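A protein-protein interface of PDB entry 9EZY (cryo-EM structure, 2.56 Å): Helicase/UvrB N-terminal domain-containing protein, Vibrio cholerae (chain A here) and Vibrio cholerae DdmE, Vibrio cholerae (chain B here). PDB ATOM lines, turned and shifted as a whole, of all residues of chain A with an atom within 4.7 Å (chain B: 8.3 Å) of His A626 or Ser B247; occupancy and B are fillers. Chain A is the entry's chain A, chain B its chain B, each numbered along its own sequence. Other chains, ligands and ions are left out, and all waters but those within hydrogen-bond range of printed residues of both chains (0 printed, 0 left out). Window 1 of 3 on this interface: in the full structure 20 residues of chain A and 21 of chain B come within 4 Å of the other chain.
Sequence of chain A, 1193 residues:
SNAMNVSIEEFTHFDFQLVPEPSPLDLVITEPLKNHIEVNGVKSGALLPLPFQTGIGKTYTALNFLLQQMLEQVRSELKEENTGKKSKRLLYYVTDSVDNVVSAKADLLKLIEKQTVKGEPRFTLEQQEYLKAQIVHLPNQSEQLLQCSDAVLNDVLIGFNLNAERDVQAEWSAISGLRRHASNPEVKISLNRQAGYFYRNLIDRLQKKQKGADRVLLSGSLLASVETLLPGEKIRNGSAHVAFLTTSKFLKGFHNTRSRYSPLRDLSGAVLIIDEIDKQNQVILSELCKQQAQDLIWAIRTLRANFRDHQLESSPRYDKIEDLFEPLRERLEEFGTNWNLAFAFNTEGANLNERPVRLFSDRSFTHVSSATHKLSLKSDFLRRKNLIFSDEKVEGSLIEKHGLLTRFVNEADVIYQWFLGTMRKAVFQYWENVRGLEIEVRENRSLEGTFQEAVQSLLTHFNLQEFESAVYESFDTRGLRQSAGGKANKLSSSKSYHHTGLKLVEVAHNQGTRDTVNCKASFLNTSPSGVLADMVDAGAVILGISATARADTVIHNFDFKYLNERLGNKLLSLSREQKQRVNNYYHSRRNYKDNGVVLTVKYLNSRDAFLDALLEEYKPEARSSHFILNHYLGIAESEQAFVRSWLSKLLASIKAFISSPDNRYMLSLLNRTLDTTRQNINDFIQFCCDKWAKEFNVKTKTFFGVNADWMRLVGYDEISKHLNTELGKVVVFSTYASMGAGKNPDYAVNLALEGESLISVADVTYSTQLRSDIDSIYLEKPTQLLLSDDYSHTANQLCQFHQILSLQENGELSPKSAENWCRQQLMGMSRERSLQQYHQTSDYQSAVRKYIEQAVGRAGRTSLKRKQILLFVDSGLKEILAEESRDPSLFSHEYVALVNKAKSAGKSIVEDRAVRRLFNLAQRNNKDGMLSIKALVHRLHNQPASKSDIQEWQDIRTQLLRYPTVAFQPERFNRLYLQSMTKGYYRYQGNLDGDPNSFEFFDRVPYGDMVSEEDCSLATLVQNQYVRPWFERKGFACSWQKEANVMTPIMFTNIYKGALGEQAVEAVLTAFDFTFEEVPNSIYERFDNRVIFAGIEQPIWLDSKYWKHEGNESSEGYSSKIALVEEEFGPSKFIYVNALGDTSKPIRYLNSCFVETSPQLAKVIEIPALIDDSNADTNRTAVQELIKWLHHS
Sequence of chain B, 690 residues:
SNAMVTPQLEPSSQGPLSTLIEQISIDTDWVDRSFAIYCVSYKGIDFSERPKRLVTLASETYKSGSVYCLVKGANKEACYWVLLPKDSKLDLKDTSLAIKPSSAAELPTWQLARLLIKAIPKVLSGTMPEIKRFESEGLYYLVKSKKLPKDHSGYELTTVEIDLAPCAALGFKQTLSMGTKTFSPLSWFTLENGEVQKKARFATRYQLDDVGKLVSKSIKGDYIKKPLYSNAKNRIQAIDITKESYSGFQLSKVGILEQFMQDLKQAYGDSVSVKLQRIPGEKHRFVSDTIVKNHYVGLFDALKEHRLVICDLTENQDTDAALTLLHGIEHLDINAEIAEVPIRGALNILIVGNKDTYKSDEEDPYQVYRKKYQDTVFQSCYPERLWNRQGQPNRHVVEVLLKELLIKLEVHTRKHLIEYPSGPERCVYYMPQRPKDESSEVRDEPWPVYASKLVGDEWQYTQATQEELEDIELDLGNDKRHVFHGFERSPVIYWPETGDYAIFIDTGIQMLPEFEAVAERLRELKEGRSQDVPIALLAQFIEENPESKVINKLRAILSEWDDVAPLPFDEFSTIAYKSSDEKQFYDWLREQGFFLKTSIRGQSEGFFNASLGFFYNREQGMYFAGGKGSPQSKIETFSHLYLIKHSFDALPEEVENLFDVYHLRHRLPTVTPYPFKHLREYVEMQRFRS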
ATOM      1  N   ASP A 612      -2.004  -9.141 -19.997  1.00  0.00           N
ATOM      2  CA  ASP A 612      -2.408  -9.996 -18.886  1.00  0.00           C
ATOM      3  C   ASP A 612      -1.529  -9.754 -17.669  1.00  0.00           C
ATOM      4  O   ASP A 612      -2.021  -9.658 -16.541  1.00  0.00           O
ATOM      5  CB  ASP A 612      -2.345 -11.464 -19.302  1.00  0.00           C
ATOM      6  CG  ASP A 612      -3.487 -11.863 -20.209  1.00  0.00           C
ATOM      7  OD1 ASP A 612      -4.507 -11.143 -20.238  1.00  0.00           O
ATOM      8  OD2 ASP A 612      -3.367 -12.901 -20.893  1.00  0.00           O
ATOM      9  N   SER A 624      -7.922 -13.648 -12.048  1.00  0.00           N
ATOM     10  CA  SER A 624      -7.985 -13.790 -13.498  1.00  0.00           C
ATOM     11  C   SER A 624      -7.894 -12.422 -14.152  1.00  0.00           C
ATOM     12  O   SER A 624      -8.580 -11.483 -13.735  1.00  0.00           O
ATOM     13  CB  SER A 624      -9.276 -14.495 -13.918  1.00  0.00           C
ATOM     14  OG  SER A 624      -9.433 -14.468 -15.325  1.00  0.00           O
ATOM     15  N   SER A 625      -7.046 -12.312 -15.178  1.00  0.00           N
ATOM     16  CA  SER A 625      -6.975 -11.076 -15.947  1.00  0.00           C
ATOM     17  C   SER A 625      -8.287 -10.794 -16.662  1.00  0.00           C
ATOM     18  O   SER A 625      -8.680  -9.631 -16.801  1.00  0.00           O
ATOM     19  CB  SER A 625      -5.827 -11.150 -16.952  1.00  0.00           C
ATOM     20  OG  SER A 625      -6.044 -12.183 -17.895  1.00  0.00           O
ATOM     21  N   HIS A 626      -8.975 -11.838 -17.128  1.00  0.00           N
ATOM     22  CA  HIS A 626     -10.282 -11.639 -17.743  1.00  0.00           C
ATOM     23  C   HIS A 626     -11.261 -11.018 -16.756  1.00  0.00           C
ATOM     24  O   HIS A 626     -11.998 -10.089 -17.103  1.00  0.00           O
ATOM     25  CB  HIS A 626     -10.826 -12.968 -18.264  1.00  0.00           C
ATOM     26  CG  HIS A 626     -10.121 -13.474 -19.484  1.00  0.00           C
ATOM     27  ND1 HIS A 626      -8.758 -13.670 -19.528  1.00  0.00           N
ATOM     28  CD2 HIS A 626     -10.593 -13.834 -20.700  1.00  0.00           C
ATOM     29  CE1 HIS A 626      -8.420 -14.123 -20.723  1.00  0.00           C
ATOM     30  NE2 HIS A 626      -9.516 -14.231 -21.452  1.00  0.00           N
ATOM     31  N   PHE A 627     -11.279 -11.515 -15.519  1.00  0.00           N
ATOM     32  CA  PHE A 627     -12.147 -10.933 -14.503  1.00  0.00           C
ATOM     33  C   PHE A 627     -11.754  -9.493 -14.201  1.00  0.00           C
ATOM     34  O   PHE A 627     -12.622  -8.624 -14.052  1.00  0.00           O
ATOM     35  CB  PHE A 627     -12.100 -11.773 -13.229  1.00  0.00           C
ATOM     36  CG  PHE A 627     -12.902 -11.199 -12.101  1.00  0.00           C
ATOM     37  CD1 PHE A 627     -14.278 -11.112 -12.186  1.00  0.00           C
ATOM     38  CD2 PHE A 627     -12.276 -10.740 -10.956  1.00  0.00           C
ATOM     39  CE1 PHE A 627     -15.016 -10.582 -11.151  1.00  0.00           C
ATOM     40  CE2 PHE A 627     -13.009 -10.209  -9.918  1.00  0.00           C
ATOM     41  CZ  PHE A 627     -14.379 -10.128 -10.015  1.00  0.00           C
ATOM     42  N   ILE A 628     -10.452  -9.221 -14.105  1.00  0.00           N
ATOM     43  CA  ILE A 628      -9.998  -7.865 -13.805  1.00  0.00           C
ATOM     44  C   ILE A 628     -10.454  -6.907 -14.896  1.00  0.00           C
ATOM     45  O   ILE A 628     -10.946  -5.808 -14.620  1.00  0.00           O
ATOM     46  CB  ILE A 628      -8.470  -7.838 -13.632  1.00  0.00           C
ATOM     47  CG1 ILE A 628      -8.059  -8.636 -12.394  1.00  0.00           C
ATOM     48  CG2 ILE A 628      -7.974  -6.408 -13.517  1.00  0.00           C
ATOM     49  CD1 ILE A 628      -6.636  -9.139 -12.441  1.00  0.00           C
ATOM     50  N   LEU A 629     -10.294  -7.311 -16.158  1.00  0.00           N
ATOM     51  CA  LEU A 629     -10.745  -6.471 -17.260  1.00  0.00           C
ATOM     52  C   LEU A 629     -12.256  -6.291 -17.230  1.00  0.00           C
ATOM     53  O   LEU A 629     -12.764  -5.187 -17.462  1.00  0.00           O
ATOM     54  CB  LEU A 629     -10.305  -7.080 -18.592  1.00  0.00           C
ATOM     55  CG  LEU A 629     -10.562  -6.230 -19.837  1.00  0.00           C
ATOM     56  CD1 LEU A 629      -9.371  -5.342 -20.134  1.00  0.00           C
ATOM     57  CD2 LEU A 629     -10.877  -7.112 -21.025  1.00  0.00           C
ATOM     58  N   ASN A 630     -12.994  -7.366 -16.952  1.00  0.00           N
ATOM     59  CA  ASN A 630     -14.451  -7.289 -16.971  1.00  0.00           C
ATOM     60  C   ASN A 630     -14.988  -6.529 -15.766  1.00  0.00           C
ATOM     61  O   ASN A 630     -15.873  -5.678 -15.900  1.00  0.00           O
ATOM     62  CB  ASN A 630     -15.043  -8.696 -17.020  1.00  0.00           C
ATOM     63  CG  ASN A 630     -16.518  -8.717 -16.687  1.00  0.00           C
ATOM     64  OD1 ASN A 630     -16.956  -9.461 -15.811  1.00  0.00           O
ATOM     65  ND2 ASN A 630     -17.294  -7.896 -17.382  1.00  0.00           N
ATOM     66  N   GLN A 640     -14.847  -7.425 -25.074  1.00  0.00           N
ATOM     67  CA  GLN A 640     -13.637  -7.765 -24.335  1.00  0.00           C
ATOM     68  C   GLN A 640     -12.460  -8.009 -25.271  1.00  0.00           C
ATOM     69  O   GLN A 640     -11.354  -7.514 -25.028  1.00  0.00           O
ATOM     70  CB  GLN A 640     -13.899  -8.991 -23.462  1.00  0.00           C
ATOM     71  CG  GLN A 640     -12.674  -9.532 -22.744  1.00  0.00           C
ATOM     72  CD  GLN A 640     -12.964  -9.927 -21.308  1.00  0.00           C
ATOM     73  OE1 GLN A 640     -14.120 -10.055 -20.906  1.00  0.00           O
ATOM     74  NE2 GLN A 640     -11.910 -10.124 -20.526  1.00  0.00           N
ATOM     75  N   ARG A 644      -9.138  -5.681 -25.366  1.00  0.00           N
ATOM     76  CA  ARG A 644      -7.836  -6.273 -25.102  1.00  0.00           C
ATOM     77  C   ARG A 644      -6.833  -5.880 -26.172  1.00  0.00           C
ATOM     78  O   ARG A 644      -5.740  -5.404 -25.850  1.00  0.00           O
ATOM     79  CB  ARG A 644      -7.959  -7.793 -25.019  1.00  0.00           C
ATOM     80  CG  ARG A 644      -8.558  -8.286 -23.716  1.00  0.00           C
ATOM     81  CD  ARG A 644      -8.689  -9.795 -23.704  1.00  0.00           C
ATOM     82  NE  ARG A 644      -7.385 -10.443 -23.719  1.00  0.00           N
ATOM     83  CZ  ARG A 644      -6.624 -10.623 -22.648  1.00  0.00           C
ATOM     84  NH1 ARG A 644      -7.008 -10.216 -21.449  1.00  0.00           N
ATOM     85  NH2 ARG A 644      -5.445 -11.222 -22.784  1.00  0.00           N
ATOM     86  N   VAL B 143     -18.012 -14.538 -11.030  1.00  0.00           N
ATOM     87  CA  VAL B 143     -17.384 -14.933 -12.278  1.00  0.00           C
ATOM     88  C   VAL B 143     -17.475 -13.834 -13.328  1.00  0.00           C
ATOM     89  O   VAL B 143     -16.637 -13.762 -14.228  1.00  0.00           O
ATOM     90  CB  VAL B 143     -18.012 -16.244 -12.801  1.00  0.00           C
ATOM     91  CG1 VAL B 143     -17.779 -16.404 -14.297  1.00  0.00           C
ATOM     92  CG2 VAL B 143     -17.463 -17.434 -12.046  1.00  0.00           C
ATOM     93  N   LYS B 144     -18.475 -12.965 -13.224  1.00  0.00           N
ATOM     94  CA  LYS B 144     -18.784 -12.051 -14.310  1.00  0.00           C
ATOM     95  C   LYS B 144     -19.780 -11.017 -13.814  1.00  0.00           C
ATOM     96  O   LYS B 144     -20.735 -11.347 -13.106  1.00  0.00           O
ATOM     97  CB  LYS B 144     -19.336 -12.828 -15.509  1.00  0.00           C
ATOM     98  CG  LYS B 144     -20.171 -12.022 -16.483  1.00  0.00           C
ATOM     99  CD  LYS B 144     -20.227 -12.694 -17.855  1.00  0.00           C
ATOM    100  CE  LYS B 144     -20.777 -14.121 -17.800  1.00  0.00           C
ATOM    101  NZ  LYS B 144     -22.180 -14.204 -18.287  1.00  0.00           N
ATOM    102  N   SER B 145     -19.547  -9.762 -14.191  1.00  0.00           N
ATOM    103  CA  SER B 145     -20.383  -8.655 -13.753  1.00  0.00           C
ATOM    104  C   SER B 145     -20.756  -7.796 -14.949  1.00  0.00           C
ATOM    105  O   SER B 145     -20.024  -7.729 -15.939  1.00  0.00           O
ATOM    106  CB  SER B 145     -19.674  -7.797 -12.697  1.00  0.00           C
ATOM    107  OG  SER B 145     -18.520  -7.178 -13.235  1.00  0.00           O
ATOM    108  N   GLN B 237     -20.126 -20.571 -18.910  1.00  0.00           N
ATOM    109  CA  GLN B 237     -19.629 -21.672 -19.720  1.00  0.00           C
ATOM    110  C   GLN B 237     -19.215 -22.842 -18.840  1.00  0.00           C
ATOM    111  O   GLN B 237     -18.659 -22.660 -17.754  1.00  0.00           O
ATOM    112  CB  GLN B 237     -18.438 -21.212 -20.559  1.00  0.00           C
ATOM    113  CG  GLN B 237     -18.675 -19.935 -21.355  1.00  0.00           C
ATOM    114  CD  GLN B 237     -17.424 -19.090 -21.480  1.00  0.00           C
ATOM    115  OE1 GLN B 237     -17.188 -18.456 -22.508  1.00  0.00           O
ATOM    116  NE2 GLN B 237     -16.607 -19.084 -20.435  1.00  0.00           N
ATOM    117  N   ASP B 240     -13.916 -23.465 -20.884  1.00  0.00           N
ATOM    118  CA  ASP B 240     -13.476 -22.409 -21.784  1.00  0.00           C
ATOM    119  C   ASP B 240     -11.962 -22.454 -21.911  1.00  0.00           C
ATOM    120  O   ASP B 240     -11.245 -22.118 -20.964  1.00  0.00           O
ATOM    121  CB  ASP B 240     -13.925 -21.032 -21.286  1.00  0.00           C
ATOM    122  CG  ASP B 240     -13.662 -19.934 -22.295  1.00  0.00           C
ATOM    123  OD1 ASP B 240     -12.996 -20.205 -23.315  1.00  0.00           O
ATOM    124  OD2 ASP B 240     -14.125 -18.796 -22.071  1.00  0.00           O
ATOM    125  N   THR B 242     -10.553 -21.134 -24.918  1.00  0.00           N
ATOM    126  CA  THR B 242     -10.586 -20.489 -26.230  1.00  0.00           C
ATOM    127  C   THR B 242      -9.204 -20.400 -26.866  1.00  0.00           C
ATOM    128  O   THR B 242      -8.987 -20.919 -27.967  1.00  0.00           O
ATOM    129  CB  THR B 242     -11.198 -19.094 -26.103  1.00  0.00           C
ATOM    130  OG1 THR B 242     -12.538 -19.202 -25.608  1.00  0.00           O
ATOM    131  CG2 THR B 242     -11.223 -18.397 -27.453  1.00  0.00           C
ATOM    132  N   LYS B 243      -8.259 -19.749 -26.196  1.00  0.00           N
ATOM    133  CA  LYS B 243      -6.890 -19.615 -26.681  1.00  0.00           C
ATOM    134  C   LYS B 243      -5.915 -20.287 -25.726  1.00  0.00           C
ATOM    135  O   LYS B 243      -4.816 -19.791 -25.479  1.00  0.00           O
ATOM    136  CB  LYS B 243      -6.518 -18.146 -26.873  1.00  0.00           C
ATOM    137  CG  LYS B 243      -7.351 -17.422 -27.917  1.00  0.00           C
ATOM    138  CD  LYS B 243      -6.635 -17.353 -29.264  1.00  0.00           C
ATOM    139  CE  LYS B 243      -7.130 -16.205 -30.142  1.00  0.00           C
ATOM    140  NZ  LYS B 243      -7.400 -14.940 -29.404  1.00  0.00           N
ATOM    141  N   GLU B 244      -6.311 -21.435 -25.178  1.00  0.00           N
ATOM    142  CA  GLU B 244      -5.552 -22.083 -24.111  1.00  0.00           C
ATOM    143  C   GLU B 244      -5.266 -21.099 -22.982  1.00  0.00           C
ATOM    144  O   GLU B 244      -4.273 -21.223 -22.261  1.00  0.00           O
ATOM    145  CB  GLU B 244      -4.250 -22.691 -24.641  1.00  0.00           C
ATOM    146  CG  GLU B 244      -4.430 -23.983 -25.429  1.00  0.00           C
ATOM    147  CD  GLU B 244      -5.276 -23.809 -26.674  1.00  0.00           C
ATOM    148  OE1 GLU B 244      -5.791 -24.822 -27.191  1.00  0.00           O
ATOM    149  OE2 GLU B 244      -5.418 -22.660 -27.142  1.00  0.00           O
ATOM    150  N   SER B 245      -6.146 -20.114 -22.822  1.00  0.00           N
ATOM    151  CA  SER B 245      -5.962 -19.073 -21.822  1.00  0.00           C
ATOM    152  C   SER B 245      -6.428 -19.583 -20.468  1.00  0.00           C
ATOM    153  O   SER B 245      -7.618 -19.857 -20.275  1.00  0.00           O
ATOM    154  CB  SER B 245      -6.732 -17.816 -22.218  1.00  0.00           C
ATOM    155  OG  SER B 245      -6.496 -16.766 -21.299  1.00  0.00           O
ATOM    156  N   TYR B 246      -5.492 -19.713 -19.527  1.00  0.00           N
ATOM    157  CA  TYR B 246      -5.853 -20.163 -18.190  1.00  0.00           C
ATOM    158  C   TYR B 246      -6.785 -19.169 -17.511  1.00  0.00           C
ATOM    159  O   TYR B 246      -7.733 -19.565 -16.824  1.00  0.00           O
ATOM    160  CB  TYR B 246      -4.595 -20.376 -17.351  1.00  0.00           C
ATOM    161  CG  TYR B 246      -4.882 -20.775 -15.926  1.00  0.00           C
ATOM    162  CD1 TYR B 246      -5.639 -21.901 -15.640  1.00  0.00           C
ATOM    163  CD2 TYR B 246      -4.395 -20.028 -14.865  1.00  0.00           C
ATOM    164  CE1 TYR B 246      -5.904 -22.271 -14.339  1.00  0.00           C
ATOM    165  CE2 TYR B 246      -4.653 -20.390 -13.561  1.00  0.00           C
ATOM    166  CZ  TYR B 246      -5.408 -21.513 -13.303  1.00  0.00           C
ATOM    167  OH  TYR B 246      -5.669 -21.878 -12.003  1.00  0.00           O
ATOM    168  N   SER B 247      -6.532 -17.872 -17.692  1.00  0.00           N
ATOM    169  CA  SER B 247      -7.368 -16.860 -17.059  1.00  0.00           C
ATOM    170  C   SER B 247      -8.815 -16.934 -17.522  1.00  0.00           C
ATOM    171  O   SER B 247      -9.722 -16.712 -16.712  1.00  0.00           O
ATOM    172  CB  SER B 247      -6.802 -15.467 -17.337  1.00  0.00           C
ATOM    173  OG  SER B 247      -6.607 -15.265 -18.724  1.00  0.00           O
ATOM    174  N   GLY B 248      -9.055 -17.233 -18.795  1.00  0.00           N
ATOM    175  CA  GLY B 248     -10.408 -17.416 -19.281  1.00  0.00           C
ATOM    176  C   GLY B 248     -10.987 -18.741 -18.833  1.00  0.00           C
ATOM    177  O   GLY B 248     -12.201 -18.878 -18.665  1.00  0.00           O
ATOM    178  N   PHE B 249     -10.114 -19.730 -18.640  1.00  0.00           N
ATOM    179  CA  PHE B 249     -10.554 -21.017 -18.115  1.00  0.00           C
ATOM    180  C   PHE B 249     -11.056 -20.880 -16.684  1.00  0.00           C
ATOM    181  O   PHE B 249     -11.988 -21.579 -16.273  1.00  0.00           O
ATOM    182  CB  PHE B 249      -9.405 -22.024 -18.197  1.00  0.00           C
ATOM    183  CG  PHE B 249      -9.638 -23.287 -17.421  1.00  0.00           C
ATOM    184  CD1 PHE B 249      -9.200 -23.402 -16.114  1.00  0.00           C
ATOM    185  CD2 PHE B 249     -10.281 -24.363 -18.002  1.00  0.00           C
ATOM    186  CE1 PHE B 249      -9.409 -24.563 -15.400  1.00  0.00           C
ATOM    187  CE2 PHE B 249     -10.491 -25.527 -17.293  1.00  0.00           C
ATOM    188  CZ  PHE B 249     -10.054 -25.627 -15.991  1.00  0.00           C
ATOM    189  N   GLN B 250     -10.450 -19.979 -15.910  1.00  0.00           N
ATOM    190  CA  GLN B 250     -10.844 -19.797 -14.518  1.00  0.00           C
ATOM    191  C   GLN B 250     -12.262 -19.263 -14.379  1.00  0.00           C
ATOM    192  O   GLN B 250     -12.847 -19.376 -13.297  1.00  0.00           O
ATOM    193  CB  GLN B 250      -9.873 -18.842 -13.826  1.00  0.00           C
ATOM    194  CG  GLN B 250      -8.545 -19.468 -13.453  1.00  0.00           C
ATOM    195  CD  GLN B 250      -7.568 -18.454 -12.900  1.00  0.00           C
ATOM    196  OE1 GLN B 250      -7.509 -17.317 -13.363  1.00  0.00           O
ATOM    197  NE2 GLN B 250      -6.797 -18.860 -11.901  1.00  0.00           N
ATOM    198  N   LEU B 251     -12.826 -18.686 -15.437  1.00  0.00           N
ATOM    199  CA  LEU B 251     -14.142 -18.065 -15.379  1.00  0.00           C
ATOM    200  C   LEU B 251     -15.250 -18.981 -15.881  1.00  0.00           C
ATOM    201  O   LEU B 251     -16.375 -18.516 -16.090  1.00  0.00           O
ATOM    202  CB  LEU B 251     -14.142 -16.762 -16.179  1.00  0.00           C
ATOM    203  CG  LEU B 251     -13.107 -15.719 -15.752  1.00  0.00           C
ATOM    204  CD1 LEU B 251     -13.347 -14.411 -16.484  1.00  0.00           C
ATOM    205  CD2 LEU B 251     -13.129 -15.503 -14.247  1.00  0.00           C
ATOM    206  N   SER B 252     -14.959 -20.258 -16.086  1.00  0.00           N
ATOM    207  CA  SER B 252     -15.975 -21.239 -16.425  1.00  0.00           C
ATOM    208  C   SER B 252     -16.425 -21.974 -15.168  1.00  0.00           C
ATOM    209  O   SER B 252     -15.787 -21.903 -14.116  1.00  0.00           O
ATOM    210  CB  SER B 252     -15.438 -22.230 -17.457  1.00  0.00           C
ATOM    211  OG  SER B 252     -14.330 -22.946 -16.943  1.00  0.00           O
ATOM    212  N   GLY B 255     -13.685 -24.245 -14.023  1.00  0.00           N
ATOM    213  CA  GLY B 255     -12.624 -23.496 -13.370  1.00  0.00           C
ATOM    214  C   GLY B 255     -13.008 -23.091 -11.960  1.00  0.00           C
ATOM    215  O   GLY B 255     -12.192 -23.150 -11.034  1.00  0.00           O
ATOM    216  N   LEU B 522      -2.880 -25.776 -18.940  1.00  0.00           N
ATOM    217  CA  LEU B 522      -3.100 -24.366 -19.228  1.00  0.00           C
ATOM    218  C   LEU B 522      -2.184 -23.484 -18.394  1.00  0.00           C
ATOM    219  O   LEU B 522      -1.674 -22.474 -18.886  1.00  0.00           O
ATOM    220  CB  LEU B 522      -4.565 -24.009 -18.981  1.00  0.00           C
ATOM    221  CG  LEU B 522      -5.562 -24.658 -19.944  1.00  0.00           C
ATOM    222  CD1 LEU B 522      -6.974 -24.527 -19.411  1.00  0.00           C
ATOM    223  CD2 LEU B 522      -5.456 -24.042 -21.324  1.00  0.00           C
ATOM    224  N   ARG B 523      -1.966 -23.842 -17.128  1.00  0.00           N
ATOM    225  CA  ARG B 523      -1.030 -23.086 -16.304  1.00  0.00           C
ATOM    226  C   ARG B 523       0.389 -23.197 -16.845  1.00  0.00           C
ATOM    227  O   ARG B 523       1.134 -22.209 -16.863  1.00  0.00           O
ATOM    228  CB  ARG B 523      -1.094 -23.571 -14.856  1.00  0.00           C
ATOM    229  CG  ARG B 523      -2.162 -22.881 -14.027  1.00  0.00           C
ATOM    230  CD  ARG B 523      -2.074 -23.272 -12.564  1.00  0.00           C
ATOM    231  NE  ARG B 523      -3.025 -24.325 -12.225  1.00  0.00           N
ATOM    232  CZ  ARG B 523      -2.708 -25.594 -11.998  1.00  0.00           C
ATOM    233  NH1 ARG B 523      -1.459 -26.025 -12.080  1.00  0.00           N
ATOM    234  NH2 ARG B 523      -3.672 -26.455 -11.684  1.00  0.00           N
ATOM    235  N   LYS B 526       0.574 -20.923 -19.721  1.00  0.00           N
ATOM    236  CA  LYS B 526       0.562 -19.540 -19.259  1.00  0.00           C
ATOM    237  C   LYS B 526       1.941 -19.113 -18.781  1.00  0.00           C
ATOM    238  O   LYS B 526       2.404 -18.010 -19.098  1.00  0.00           O
ATOM    239  CB  LYS B 526      -0.467 -19.387 -18.140  1.00  0.00           C
ATOM    240  CG  LYS B 526      -0.650 -17.974 -17.613  1.00  0.00           C
ATOM    241  CD  LYS B 526      -0.755 -17.977 -16.094  1.00  0.00           C
ATOM    242  CE  LYS B 526      -1.403 -16.712 -15.547  1.00  0.00           C
ATOM    243  NZ  LYS B 526      -1.427 -15.588 -16.523  1.00  0.00           N
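Among the printed residues, pairs that only touch across the chains: Ser A624 with Gln B250 (3.4 Å), Ser A624 with Leu B251 (3.9 Å), His A626 with Ser B245 (3.3 Å), His A626 with Gly B248 (3.6 Å), His A626 with Leu B251 (3.4 Å), Phe A627 with Leu B251 (3.7 Å) and Asn A630 with Lys B144 (3.5 Å).
His A626 touches four residues of chain B. Printed residues of chain A within 4 Å of Ser B247: Ser A624, Ser A625 and His A626. Ser A625 touches just one residue of chain B: Ser B247 (3.2 Å). Of the printed residues of chain A, Gly B248 touches His A626 (3.6 Å). Of the printed residues of chain B, Ser A624 touches Ser B247, Gln B250 and Leu B251. Of the printed residues of chain A, Leu B251 touches Ser A624, His A626 and Phe A627. Gln A640 touches none of the printed residues of chain B. Leu A629 touches none of the printed residues of chain B. The nearest residue of chain A that does not touch Ser B247 is Asp A612 (4.6 Å).
The backbone NH of Ser B145 lies within hydrogen-bond range of the side-chain amide oxygen of Asn A630. The side-chain hydroxyl of Ser A624 sits at hydrogen-bond distance from the backbone carbonyl oxygen of Ser B247 (2.7 Å). The side-chain hydroxyl (OG) of Ser A625 is in hydrogen-bond range of the side-chain hydroxyl (OG) of Ser B247 (3.2 Å). The side-chain hydroxyl of Ser B247 is in hydrogen-bond range of a ring nitrogen (ND1) of His A626 (2.8 Å).
Hydrophobic or aromatic side chains of chain A that line the printed part of chain B: His A626. Among the printed residues, 11 pairs touch across the chains.
OH of Tyr B246 lies close to NE2 of Gln B250. The side-chain amide nitrogen (NE2) of Gln A640 lies within hydrogen-bond range of the backbone carbonyl oxygen (O) of His A626, 3.4 Å away. OG of Ser A625 sits at hydrogen-bond distance from ND1 of His A626, 3.5 Å away. N of His A626 sits close to OG of Ser A624 (3.2 Å). The side-chain hydroxyl (OG) of Ser A624 sits at hydrogen-bond distance from the backbone NH (N) of Phe A627 (3.5 Å). The side-chain hydroxyl of Ser B245 sits at hydrogen-bond distance from the side-chain hydroxyl of Ser B247 (3.0 Å).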
